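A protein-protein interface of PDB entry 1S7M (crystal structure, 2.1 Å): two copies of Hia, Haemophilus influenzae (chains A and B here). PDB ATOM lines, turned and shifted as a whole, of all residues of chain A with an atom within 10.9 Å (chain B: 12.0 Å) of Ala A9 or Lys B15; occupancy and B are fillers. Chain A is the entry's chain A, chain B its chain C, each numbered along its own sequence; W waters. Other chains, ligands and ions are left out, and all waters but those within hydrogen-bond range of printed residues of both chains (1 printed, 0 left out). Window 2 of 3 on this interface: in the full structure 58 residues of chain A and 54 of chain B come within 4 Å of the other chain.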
ATOM      1  N   GLY A   8      -5.872  -7.578  -7.407  1.00  0.00           N
ATOM      2  CA  GLY A   8      -5.086  -7.730  -8.679  1.00  0.00           C
ATOM      3  C   GLY A   8      -5.618  -6.906  -9.851  1.00  0.00           C
ATOM      4  O   GLY A   8      -4.966  -6.817 -10.895  1.00  0.00           O
ATOM      5  N   ALA A   9      -6.794  -6.304  -9.689  1.00  0.00           N
ATOM      6  CA  ALA A   9      -7.380  -5.500 -10.754  1.00  0.00           C
ATOM      7  C   ALA A   9      -6.632  -4.190 -10.932  1.00  0.00           C
ATOM      8  O   ALA A   9      -6.139  -3.607  -9.964  1.00  0.00           O
ATOM      9  CB  ALA A   9      -8.858  -5.212 -10.457  1.00  0.00           C
ATOM     10  N   LYS A  10      -6.536  -3.730 -12.172  1.00  0.00           N
ATOM     11  CA  LYS A  10      -5.875  -2.467 -12.438  1.00  0.00           C
ATOM     12  C   LYS A  10      -6.678  -1.641 -13.434  1.00  0.00           C
ATOM     13  O   LYS A  10      -7.416  -2.184 -14.257  1.00  0.00           O
ATOM     14  CB  LYS A  10      -4.457  -2.687 -12.977  1.00  0.00           C
ATOM     15  CG  LYS A  10      -4.371  -3.337 -14.349  1.00  0.00           C
ATOM     16  CD  LYS A  10      -2.924  -3.386 -14.815  1.00  0.00           C
ATOM     17  CE  LYS A  10      -2.813  -3.837 -16.266  1.00  0.00           C
ATOM     18  NZ  LYS A  10      -1.394  -3.859 -16.729  1.00  0.00           N
ATOM     19  N   THR A  11      -6.532  -0.328 -13.337  1.00  0.00           N
ATOM     20  CA  THR A  11      -7.207   0.598 -14.219  1.00  0.00           C
ATOM     21  C   THR A  11      -6.135   1.443 -14.886  1.00  0.00           C
ATOM     22  O   THR A  11      -5.382   2.138 -14.209  1.00  0.00           O
ATOM     23  CB  THR A  11      -8.146   1.517 -13.434  1.00  0.00           C
ATOM     24  OG1 THR A  11      -9.278   0.767 -12.991  1.00  0.00           O
ATOM     25  CG2 THR A  11      -8.606   2.687 -14.292  1.00  0.00           C
ATOM     26  N   GLU A  12      -6.056   1.375 -16.209  1.00  0.00           N
ATOM     27  CA  GLU A  12      -5.068   2.145 -16.949  1.00  0.00           C
ATOM     28  C   GLU A  12      -5.703   3.256 -17.757  1.00  0.00           C
ATOM     29  O   GLU A  12      -6.773   3.077 -18.338  1.00  0.00           O
ATOM     30  CB  GLU A  12      -4.288   1.248 -17.906  1.00  0.00           C
ATOM     31  CG  GLU A  12      -3.475   0.173 -17.236  1.00  0.00           C
ATOM     32  CD  GLU A  12      -2.396  -0.397 -18.151  1.00  0.00           C
ATOM     33  OE1 GLU A  12      -2.092   0.244 -19.191  1.00  0.00           O
ATOM     34  OE2 GLU A  12      -1.844  -1.472 -17.819  1.00  0.00           O
ATOM     35  N   ILE A  13      -5.030   4.400 -17.781  1.00  0.00           N
ATOM     36  CA  ILE A  13      -5.459   5.553 -18.549  1.00  0.00           C
ATOM     37  C   ILE A  13      -4.289   5.890 -19.467  1.00  0.00           C
ATOM     38  O   ILE A  13      -3.164   6.087 -19.008  1.00  0.00           O
ATOM     39  CB  ILE A  13      -5.736   6.773 -17.663  1.00  0.00           C
ATOM     40  CG1 ILE A  13      -6.912   6.495 -16.735  1.00  0.00           C
ATOM     41  CG2 ILE A  13      -6.032   7.980 -18.524  1.00  0.00           C
ATOM     42  CD1 ILE A  13      -7.159   7.598 -15.739  1.00  0.00           C
ATOM     43  N   LEU A  18      -9.624   4.503 -21.199  1.00  0.00           N
ATOM     44  CA  LEU A  18      -9.626   3.900 -19.878  1.00  0.00           C
ATOM     45  C   LEU A  18      -9.862   2.396 -19.967  1.00  0.00           C
ATOM     46  O   LEU A  18     -10.903   1.968 -20.450  1.00  0.00           O
ATOM     47  CB  LEU A  18     -10.747   4.533 -19.047  1.00  0.00           C
ATOM     48  CG  LEU A  18     -10.963   4.093 -17.597  1.00  0.00           C
ATOM     49  CD1 LEU A  18      -9.851   4.657 -16.736  1.00  0.00           C
ATOM     50  CD2 LEU A  18     -12.298   4.618 -17.087  1.00  0.00           C
ATOM     51  N   THR A  19      -8.915   1.595 -19.488  1.00  0.00           N
ATOM     52  CA  THR A  19      -9.068   0.141 -19.494  1.00  0.00           C
ATOM     53  C   THR A  19      -8.929  -0.460 -18.080  1.00  0.00           C
ATOM     54  O   THR A  19      -7.989  -0.133 -17.347  1.00  0.00           O
ATOM     55  CB  THR A  19      -8.015  -0.542 -20.392  1.00  0.00           C
ATOM     56  OG1 THR A  19      -8.072   0.003 -21.712  1.00  0.00           O
ATOM     57  CG2 THR A  19      -8.281  -2.019 -20.481  1.00  0.00           C
ATOM     58  N   ILE A  20      -9.870  -1.326 -17.703  1.00  0.00           N
ATOM     59  CA  ILE A  20      -9.841  -2.004 -16.413  1.00  0.00           C
ATOM     60  C   ILE A  20      -9.592  -3.476 -16.701  1.00  0.00           C
ATOM     61  O   ILE A  20     -10.352  -4.113 -17.433  1.00  0.00           O
ATOM     62  CB  ILE A  20     -11.190  -1.939 -15.630  1.00  0.00           C
ATOM     63  CG1 ILE A  20     -11.475  -0.532 -15.098  1.00  0.00           C
ATOM     64  CG2 ILE A  20     -11.124  -2.859 -14.425  1.00  0.00           C
ATOM     65  CD1 ILE A  20     -12.010   0.450 -16.102  1.00  0.00           C
ATOM     66  N   THR A  21      -8.522  -4.015 -16.138  1.00  0.00           N
ATOM     67  CA  THR A  21      -8.208  -5.421 -16.314  1.00  0.00           C
ATOM     68  C   THR A  21      -8.562  -6.105 -14.996  1.00  0.00           C
ATOM     69  O   THR A  21      -8.013  -5.774 -13.951  1.00  0.00           O
ATOM     70  CB  THR A  21      -6.719  -5.622 -16.613  1.00  0.00           C
ATOM     71  OG1 THR A  21      -6.346  -4.816 -17.735  1.00  0.00           O
ATOM     72  CG2 THR A  21      -6.432  -7.078 -16.914  1.00  0.00           C
ATOM     73  N   PRO A  22      -9.507  -7.053 -15.027  1.00  0.00           N
ATOM     74  CA  PRO A  22      -9.936  -7.777 -13.825  1.00  0.00           C
ATOM     75  C   PRO A  22      -8.768  -8.507 -13.170  1.00  0.00           C
ATOM     76  O   PRO A  22      -7.711  -8.680 -13.782  1.00  0.00           O
ATOM     77  CB  PRO A  22     -10.977  -8.753 -14.360  1.00  0.00           C
ATOM     78  CG  PRO A  22     -11.491  -8.087 -15.575  1.00  0.00           C
ATOM     79  CD  PRO A  22     -10.241  -7.533 -16.207  1.00  0.00           C
ATOM     80  N   ALA A  23      -8.963  -8.947 -11.933  1.00  0.00           N
ATOM     81  CA  ALA A  23      -7.904  -9.656 -11.224  1.00  0.00           C
ATOM     82  C   ALA A  23      -7.489 -10.919 -11.961  1.00  0.00           C
ATOM     83  O   ALA A  23      -6.460 -11.505 -11.645  1.00  0.00           O
ATOM     84  CB  ALA A  23      -8.354 -10.008  -9.806  1.00  0.00           C
ATOM     85  N   ASN A  24      -8.274 -11.325 -12.957  1.00  0.00           N
ATOM     86  CA  ASN A  24      -7.981 -12.540 -13.711  1.00  0.00           C
ATOM     87  C   ASN A  24      -7.364 -12.370 -15.108  1.00  0.00           C
ATOM     88  O   ASN A  24      -7.403 -13.296 -15.912  1.00  0.00           O
ATOM     89  CB  ASN A  24      -9.244 -13.385 -13.808  1.00  0.00           C
ATOM     90  N   GLY A  25      -6.800 -11.205 -15.409  1.00  0.00           N
ATOM     91  CA  GLY A  25      -6.187 -11.014 -16.716  1.00  0.00           C
ATOM     92  C   GLY A  25      -7.090 -10.441 -17.795  1.00  0.00           C
ATOM     93  O   GLY A  25      -8.316 -10.488 -17.682  1.00  0.00           O
ATOM     94  N   ALA A  26      -6.475  -9.907 -18.850  1.00  0.00           N
ATOM     95  CA  ALA A  26      -7.200  -9.301 -19.963  1.00  0.00           C
ATOM     96  C   ALA A  26      -7.952 -10.324 -20.804  1.00  0.00           C
ATOM     97  O   ALA A  26      -8.725  -9.967 -21.692  1.00  0.00           O
ATOM     98  CB  ALA A  26      -6.232  -8.513 -20.847  1.00  0.00           C
ATOM     99  N   ASN A  32     -11.886  -9.853 -21.631  1.00  0.00           N
ATOM    100  CA  ASN A  32     -12.270  -9.739 -20.228  1.00  0.00           C
ATOM    101  C   ASN A  32     -12.144  -8.315 -19.743  1.00  0.00           C
ATOM    102  O   ASN A  32     -12.604  -7.974 -18.662  1.00  0.00           O
ATOM    103  CB  ASN A  32     -11.408 -10.624 -19.342  1.00  0.00           C
ATOM    104  CG  ASN A  32     -11.924 -12.032 -19.259  1.00  0.00           C
ATOM    105  OD1 ASN A  32     -13.126 -12.258 -19.106  1.00  0.00           O
ATOM    106  ND2 ASN A  32     -11.018 -12.995 -19.347  1.00  0.00           N
ATOM    107  N   THR A  33     -11.506  -7.489 -20.556  1.00  0.00           N
ATOM    108  CA  THR A  33     -11.299  -6.094 -20.234  1.00  0.00           C
ATOM    109  C   THR A  33     -12.579  -5.271 -20.246  1.00  0.00           C
ATOM    110  O   THR A  33     -13.484  -5.515 -21.036  1.00  0.00           O
ATOM    111  CB  THR A  33     -10.310  -5.469 -21.237  1.00  0.00           C
ATOM    112  OG1 THR A  33      -8.966  -5.775 -20.845  1.00  0.00           O
ATOM    113  CG2 THR A  33     -10.499  -3.974 -21.313  1.00  0.00           C
ATOM    114  N   ILE A  34     -12.656  -4.303 -19.348  1.00  0.00           N
ATOM    115  CA  ILE A  34     -13.792  -3.400 -19.306  1.00  0.00           C
ATOM    116  C   ILE A  34     -13.153  -2.086 -19.753  1.00  0.00           C
ATOM    117  O   ILE A  34     -12.204  -1.595 -19.119  1.00  0.00           O
ATOM    118  CB  ILE A  34     -14.343  -3.216 -17.892  1.00  0.00           C
ATOM    119  CG1 ILE A  34     -14.436  -4.574 -17.182  1.00  0.00           C
ATOM    120  CG2 ILE A  34     -15.698  -2.504 -17.963  1.00  0.00           C
ATOM    121  CD1 ILE A  34     -15.431  -5.493 -17.746  1.00  0.00           C
ATOM    122  N   GLN A  46     -19.362  -8.786 -19.566  1.00  0.00           N
ATOM    123  CA  GLN A  46     -20.400  -8.497 -18.587  1.00  0.00           C
ATOM    124  C   GLN A  46     -21.548  -7.735 -19.258  1.00  0.00           C
ATOM    125  O   GLN A  46     -21.628  -7.685 -20.489  1.00  0.00           O
ATOM    126  CB  GLN A  46     -19.822  -7.674 -17.450  1.00  0.00           C
ATOM    127  CG  GLN A  46     -18.544  -8.258 -16.872  1.00  0.00           C
ATOM    128  CD  GLN A  46     -18.651  -8.504 -15.392  1.00  0.00           C
ATOM    129  OE1 GLN A  46     -17.673  -8.370 -14.665  1.00  0.00           O
ATOM    130  NE2 GLN A  46     -19.838  -8.873 -14.935  1.00  0.00           N
ATOM    131  N   THR B  11     -16.943  12.206  -8.423  1.00  0.00           N
ATOM    132  CA  THR B  11     -16.271  11.213  -9.253  1.00  0.00           C
ATOM    133  C   THR B  11     -15.124  10.530  -8.510  1.00  0.00           C
ATOM    134  O   THR B  11     -14.252  11.194  -7.953  1.00  0.00           O
ATOM    135  CB  THR B  11     -15.729  11.866 -10.527  1.00  0.00           C
ATOM    136  OG1 THR B  11     -16.826  12.375 -11.286  1.00  0.00           O
ATOM    137  CG2 THR B  11     -14.968  10.857 -11.371  1.00  0.00           C
ATOM    138  N   GLU B  12     -15.114   9.200  -8.529  1.00  0.00           N
ATOM    139  CA  GLU B  12     -14.095   8.432  -7.821  1.00  0.00           C
ATOM    140  C   GLU B  12     -13.438   7.357  -8.686  1.00  0.00           C
ATOM    141  O   GLU B  12     -14.116   6.621  -9.405  1.00  0.00           O
ATOM    142  CB  GLU B  12     -14.724   7.773  -6.582  1.00  0.00           C
ATOM    143  CG  GLU B  12     -15.393   8.750  -5.603  1.00  0.00           C
ATOM    144  CD  GLU B  12     -16.172   8.049  -4.483  1.00  0.00           C
ATOM    145  OE1 GLU B  12     -17.171   7.356  -4.786  1.00  0.00           O
ATOM    146  OE2 GLU B  12     -15.792   8.188  -3.300  1.00  0.00           O
ATOM    147  N   ILE B  13     -12.116   7.253  -8.605  1.00  0.00           N
ATOM    148  CA  ILE B  13     -11.406   6.250  -9.380  1.00  0.00           C
ATOM    149  C   ILE B  13     -10.565   5.362  -8.486  1.00  0.00           C
ATOM    150  O   ILE B  13      -9.999   5.834  -7.510  1.00  0.00           O
ATOM    151  CB  ILE B  13     -10.444   6.879 -10.389  1.00  0.00           C
ATOM    152  CG1 ILE B  13     -11.111   8.043 -11.103  1.00  0.00           C
ATOM    153  CG2 ILE B  13     -10.025   5.831 -11.402  1.00  0.00           C
ATOM    154  CD1 ILE B  13     -10.277   8.633 -12.215  1.00  0.00           C
ATOM    155  N   ASN B  14     -10.486   4.077  -8.814  1.00  0.00           N
ATOM    156  CA  ASN B  14      -9.652   3.156  -8.062  1.00  0.00           C
ATOM    157  C   ASN B  14      -9.291   1.996  -8.950  1.00  0.00           C
ATOM    158  O   ASN B  14      -9.643   1.986 -10.127  1.00  0.00           O
ATOM    159  CB  ASN B  14     -10.321   2.666  -6.769  1.00  0.00           C
ATOM    160  CG  ASN B  14     -11.580   1.870  -7.018  1.00  0.00           C
ATOM    161  OD1 ASN B  14     -11.599   0.946  -7.830  1.00  0.00           O
ATOM    162  ND2 ASN B  14     -12.639   2.215  -6.302  1.00  0.00           N
ATOM    163  N   LYS B  15      -8.585   1.020  -8.388  1.00  0.00           N
ATOM    164  CA  LYS B  15      -8.131  -0.128  -9.157  1.00  0.00           C
ATOM    165  C   LYS B  15      -9.238  -0.894  -9.858  1.00  0.00           C
ATOM    166  O   LYS B  15      -8.990  -1.559 -10.864  1.00  0.00           O
ATOM    167  CB  LYS B  15      -7.342  -1.081  -8.262  1.00  0.00           C
ATOM    168  CG  LYS B  15      -8.157  -1.784  -7.203  1.00  0.00           C
ATOM    169  CD  LYS B  15      -7.281  -2.802  -6.481  1.00  0.00           C
ATOM    170  CE  LYS B  15      -8.105  -3.846  -5.741  1.00  0.00           C
ATOM    171  NZ  LYS B  15      -9.061  -3.213  -4.800  1.00  0.00           N
ATOM    172  N   ASP B  16     -10.454  -0.799  -9.331  1.00  0.00           N
ATOM    173  CA  ASP B  16     -11.579  -1.511  -9.914  1.00  0.00           C
ATOM    174  C   ASP B  16     -12.345  -0.725 -10.973  1.00  0.00           C
ATOM    175  O   ASP B  16     -13.223  -1.276 -11.633  1.00  0.00           O
ATOM    176  CB  ASP B  16     -12.534  -1.973  -8.817  1.00  0.00           C
ATOM    177  CG  ASP B  16     -11.897  -2.980  -7.891  1.00  0.00           C
ATOM    178  OD1 ASP B  16     -11.263  -3.935  -8.396  1.00  0.00           O
ATOM    179  OD2 ASP B  16     -12.032  -2.818  -6.659  1.00  0.00           O
ATOM    180  N   GLY B  17     -12.012   0.548 -11.147  1.00  0.00           N
ATOM    181  CA  GLY B  17     -12.694   1.338 -12.159  1.00  0.00           C
ATOM    182  C   GLY B  17     -13.130   2.725 -11.738  1.00  0.00           C
ATOM    183  O   GLY B  17     -12.668   3.264 -10.721  1.00  0.00           O
ATOM    184  N   LEU B  18     -14.044   3.295 -12.516  1.00  0.00           N
ATOM    185  CA  LEU B  18     -14.538   4.646 -12.278  1.00  0.00           C
ATOM    186  C   LEU B  18     -16.017   4.673 -11.932  1.00  0.00           C
ATOM    187  O   LEU B  18     -16.819   3.939 -12.515  1.00  0.00           O
ATOM    188  CB  LEU B  18     -14.271   5.499 -13.519  1.00  0.00           C
ATOM    189  CG  LEU B  18     -15.087   6.763 -13.772  1.00  0.00           C
ATOM    190  CD1 LEU B  18     -14.573   7.919 -12.949  1.00  0.00           C
ATOM    191  CD2 LEU B  18     -15.016   7.083 -15.255  1.00  0.00           C
ATOM    192  N   THR B  19     -16.370   5.536 -10.984  1.00  0.00           N
ATOM    193  CA  THR B  19     -17.750   5.664 -10.539  1.00  0.00           C
ATOM    194  C   THR B  19     -18.145   7.115 -10.352  1.00  0.00           C
ATOM    195  O   THR B  19     -17.407   7.916  -9.787  1.00  0.00           O
ATOM    196  CB  THR B  19     -17.987   4.933  -9.196  1.00  0.00           C
ATOM    197  OG1 THR B  19     -17.700   3.539  -9.339  1.00  0.00           O
ATOM    198  CG2 THR B  19     -19.431   5.079  -8.763  1.00  0.00           C
ATOM    199  N   SER B  35     -21.124   3.965 -14.045  1.00  0.00           N
ATOM    200  CA  SER B  35     -19.784   3.460 -13.848  1.00  0.00           C
ATOM    201  C   SER B  35     -19.234   2.490 -14.880  1.00  0.00           C
ATOM    202  O   SER B  35     -19.968   1.879 -15.664  1.00  0.00           O
ATOM    203  CB  SER B  35     -19.709   2.808 -12.480  1.00  0.00           C
ATOM    204  OG  SER B  35     -20.553   1.676 -12.445  1.00  0.00           O
ATOM    205  N   VAL B  36     -17.914   2.363 -14.849  1.00  0.00           N
ATOM    206  CA  VAL B  36     -17.165   1.470 -15.716  1.00  0.00           C
ATOM    207  C   VAL B  36     -16.155   0.826 -14.764  1.00  0.00           C
ATOM    208  O   VAL B  36     -15.119   1.412 -14.431  1.00  0.00           O
ATOM    209  CB  VAL B  36     -16.420   2.241 -16.814  1.00  0.00           C
ATOM    210  CG1 VAL B  36     -15.669   1.271 -17.694  1.00  0.00           C
ATOM    211  CG2 VAL B  36     -17.409   3.061 -17.636  1.00  0.00           C
ATOM    212  N   THR B  37     -16.470  -0.385 -14.326  1.00  0.00           N
ATOM    213  CA  THR B  37     -15.627  -1.079 -13.370  1.00  0.00           C
ATOM    214  C   THR B  37     -15.474  -2.542 -13.727  1.00  0.00           C
ATOM    215  O   THR B  37     -16.014  -3.009 -14.722  1.00  0.00           O
ATOM    216  CB  THR B  37     -16.238  -0.998 -11.969  1.00  0.00           C
ATOM    217  OG1 THR B  37     -17.324  -1.922 -11.884  1.00  0.00           O
ATOM    218  CG2 THR B  37     -16.797   0.383 -11.706  1.00  0.00           C
ATOM    219  N   LYS B  38     -14.765  -3.278 -12.886  1.00  0.00           N
ATOM    220  CA  LYS B  38     -14.540  -4.695 -13.126  1.00  0.00           C
ATOM    221  C   LYS B  38     -15.841  -5.496 -13.168  1.00  0.00           C
ATOM    222  O   LYS B  38     -15.873  -6.595 -13.711  1.00  0.00           O
ATOM    223  CB  LYS B  38     -13.620  -5.272 -12.049  1.00  0.00           C
ATOM    224  CG  LYS B  38     -14.248  -5.287 -10.674  1.00  0.00           C
ATOM    225  CD  LYS B  38     -13.439  -6.103  -9.704  1.00  0.00           C
ATOM    226  CE  LYS B  38     -14.300  -6.473  -8.508  1.00  0.00           C
ATOM    227  NZ  LYS B  38     -14.925  -5.267  -7.926  1.00  0.00           N
ATOM    228  N   ASP B  39     -16.914  -4.948 -12.614  1.00  0.00           N
ATOM    229  CA  ASP B  39     -18.188  -5.657 -12.615  1.00  0.00           C
ATOM    230  C   ASP B  39     -19.053  -5.327 -13.837  1.00  0.00           C
ATOM    231  O   ASP B  39     -20.196  -5.783 -13.958  1.00  0.00           O
ATOM    232  CB  ASP B  39     -18.954  -5.353 -11.323  1.00  0.00           C
ATOM    233  CG  ASP B  39     -18.210  -5.834 -10.076  1.00  0.00           C
ATOM    234  OD1 ASP B  39     -17.758  -7.003 -10.059  1.00  0.00           O
ATOM    235  OD2 ASP B  39     -18.076  -5.050  -9.119  1.00  0.00           O
ATOM    236  N   GLY B  40     -18.494  -4.541 -14.750  1.00  0.00           N
ATOM    237  CA  GLY B  40     -19.229  -4.172 -15.937  1.00  0.00           C
ATOM    238  C   GLY B  40     -19.545  -2.695 -15.992  1.00  0.00           C
ATOM    239  O   GLY B  40     -18.794  -1.860 -15.486  1.00  0.00           O
HETATM  240  O   HOH W   1     -22.445  -6.772 -15.428  1.00  0.00           O
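The side-chain amide oxygen (OE1) of Gln A46 lies close to the backbone carbonyl oxygen (O) of Lys B38, at 2.7 Å.
O of Asp B39 lies within hydrogen-bond range of NE2 of Gln A46, at 3.3 Å.
The side-chain hydroxyl of Thr A11 is in hydrogen-bond range of the backbone NH of Gly B17 (3.3 Å).
OG1 of Thr A11 lies within hydrogen-bond range of O of Lys B15 (3.2 Å).
The backbone carbonyl oxygen (O) of Asn B14 lies within hydrogen-bond range of the side-chain hydroxyl (OG1) of Thr A11 (3.1 Å).
The side-chain amide oxygen of Asn B14 is in hydrogen-bond range of the backbone NH of Gly B17 (3.4 Å).
N of Ile A20 sits at hydrogen-bond distance from O of Ile A34.
The side-chain amino group (NZ) of Lys A10 is in salt-bridge range of the side-chain carboxylate (OE2) of Glu A12, at 2.7 Å.
The side-chain amino group (NZ) of Lys B15 is in salt-bridge range of the side-chain carboxylate (OD2) of Asp B16, at 3.5 Å.
The backbone carbonyl oxygen (O) of Lys A10 is in hydrogen-bond range of the backbone NH (N) of Thr A21, at 2.8 Å.
The side-chain amino group of Lys B38 is in salt-bridge range of the side-chain carboxylate of Asp B39 (3.4 Å).
Among the printed residues, pairs that only touch across the chains: Ala A9 with Lys B15 (3.3 Å), Ile A34 with Thr B37 (3.3 Å), Ala A9 with Asp B16 (3.4 Å), Lys A10 with Lys B15 (3.5 Å), Ile A20 with Val B36 (3.7 Å), Ile A20 with Gly B17 (3.7 Å), Ile A34 with Val B36 (3.8 Å), Ile A20 with Asp B16 (3.8 Å), Gln A46 with Gly B40 (3.9 Å), Thr A11 with Asp B16 (3.96 Å) and Ile A20 with Lys B38 (3.98 Å).
No residue of chain B comes within 4 Å of Gly A8.
Of chain B, only Lys B15 (3.3 Å) and Asp B16 (3.4 Å) come within 4 Å of Ala A9.
Lys A10 touches one residue of chain B.
Of the printed residues of chain B, Thr A11 touches Asn B14, Lys B15, Asp B16 and Gly B17.
Ile A20 touches four residues of chain B.
Thr A21 touches none of the printed residues of chain B.
No residue of chain B comes within 4 Å of Pro A22.
No residue of chain B comes within 4 Å of Ala A23.
Gly A25 touches none of the printed residues of chain B.
Asn B14 touches just one residue of chain A: Thr A11.
Printed residues of chain A within 4 Å of Lys B15: Ala A9, Lys A10 and Thr A11.
Asp B16 touches just these residues of chain A: Ala A9 (3.4 Å), Thr A11 (3.96 Å) and Ile A20 (3.8 Å).
Of chain A, only Thr A11 and Ile A20 come within 4 Å of Gly B17.
Printed residues of chain A within 4 Å of Val B36: Ile A20 (3.7 Å) and Ile A34 (3.8 Å).
Of the printed residues of chain A, Lys B38 touches Ile A20 and Gln A46.
Printed residues of chain A within 4 Å of Asp B39: Gln A46 (3.3 Å).
Printed residues of chain B that touch a printed residue of chain A: Asn B14, Lys B15, Asp B16, Gly B17, Val B36, Thr B37, Lys B38, Asp B39 and Gly B40.
Hydrophobic or aromatic side chains of chain B that line the printed part of chain A: Val B36.
Printed residues of chain A that touch a printed residue of chain B: Ala A9, Lys A10, Thr A11, Ile A20, Ile A34 and Gln A46.
Hydrophobic or aromatic side chains of chain A that line the printed part of chain B: Ala A9, Ile A20 and Ile A34.
Positions printed for both chains: 11, 12, 13, 18 and 19.
Water W1 bridges O of Asp B39 and NE2 of Gln A46.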
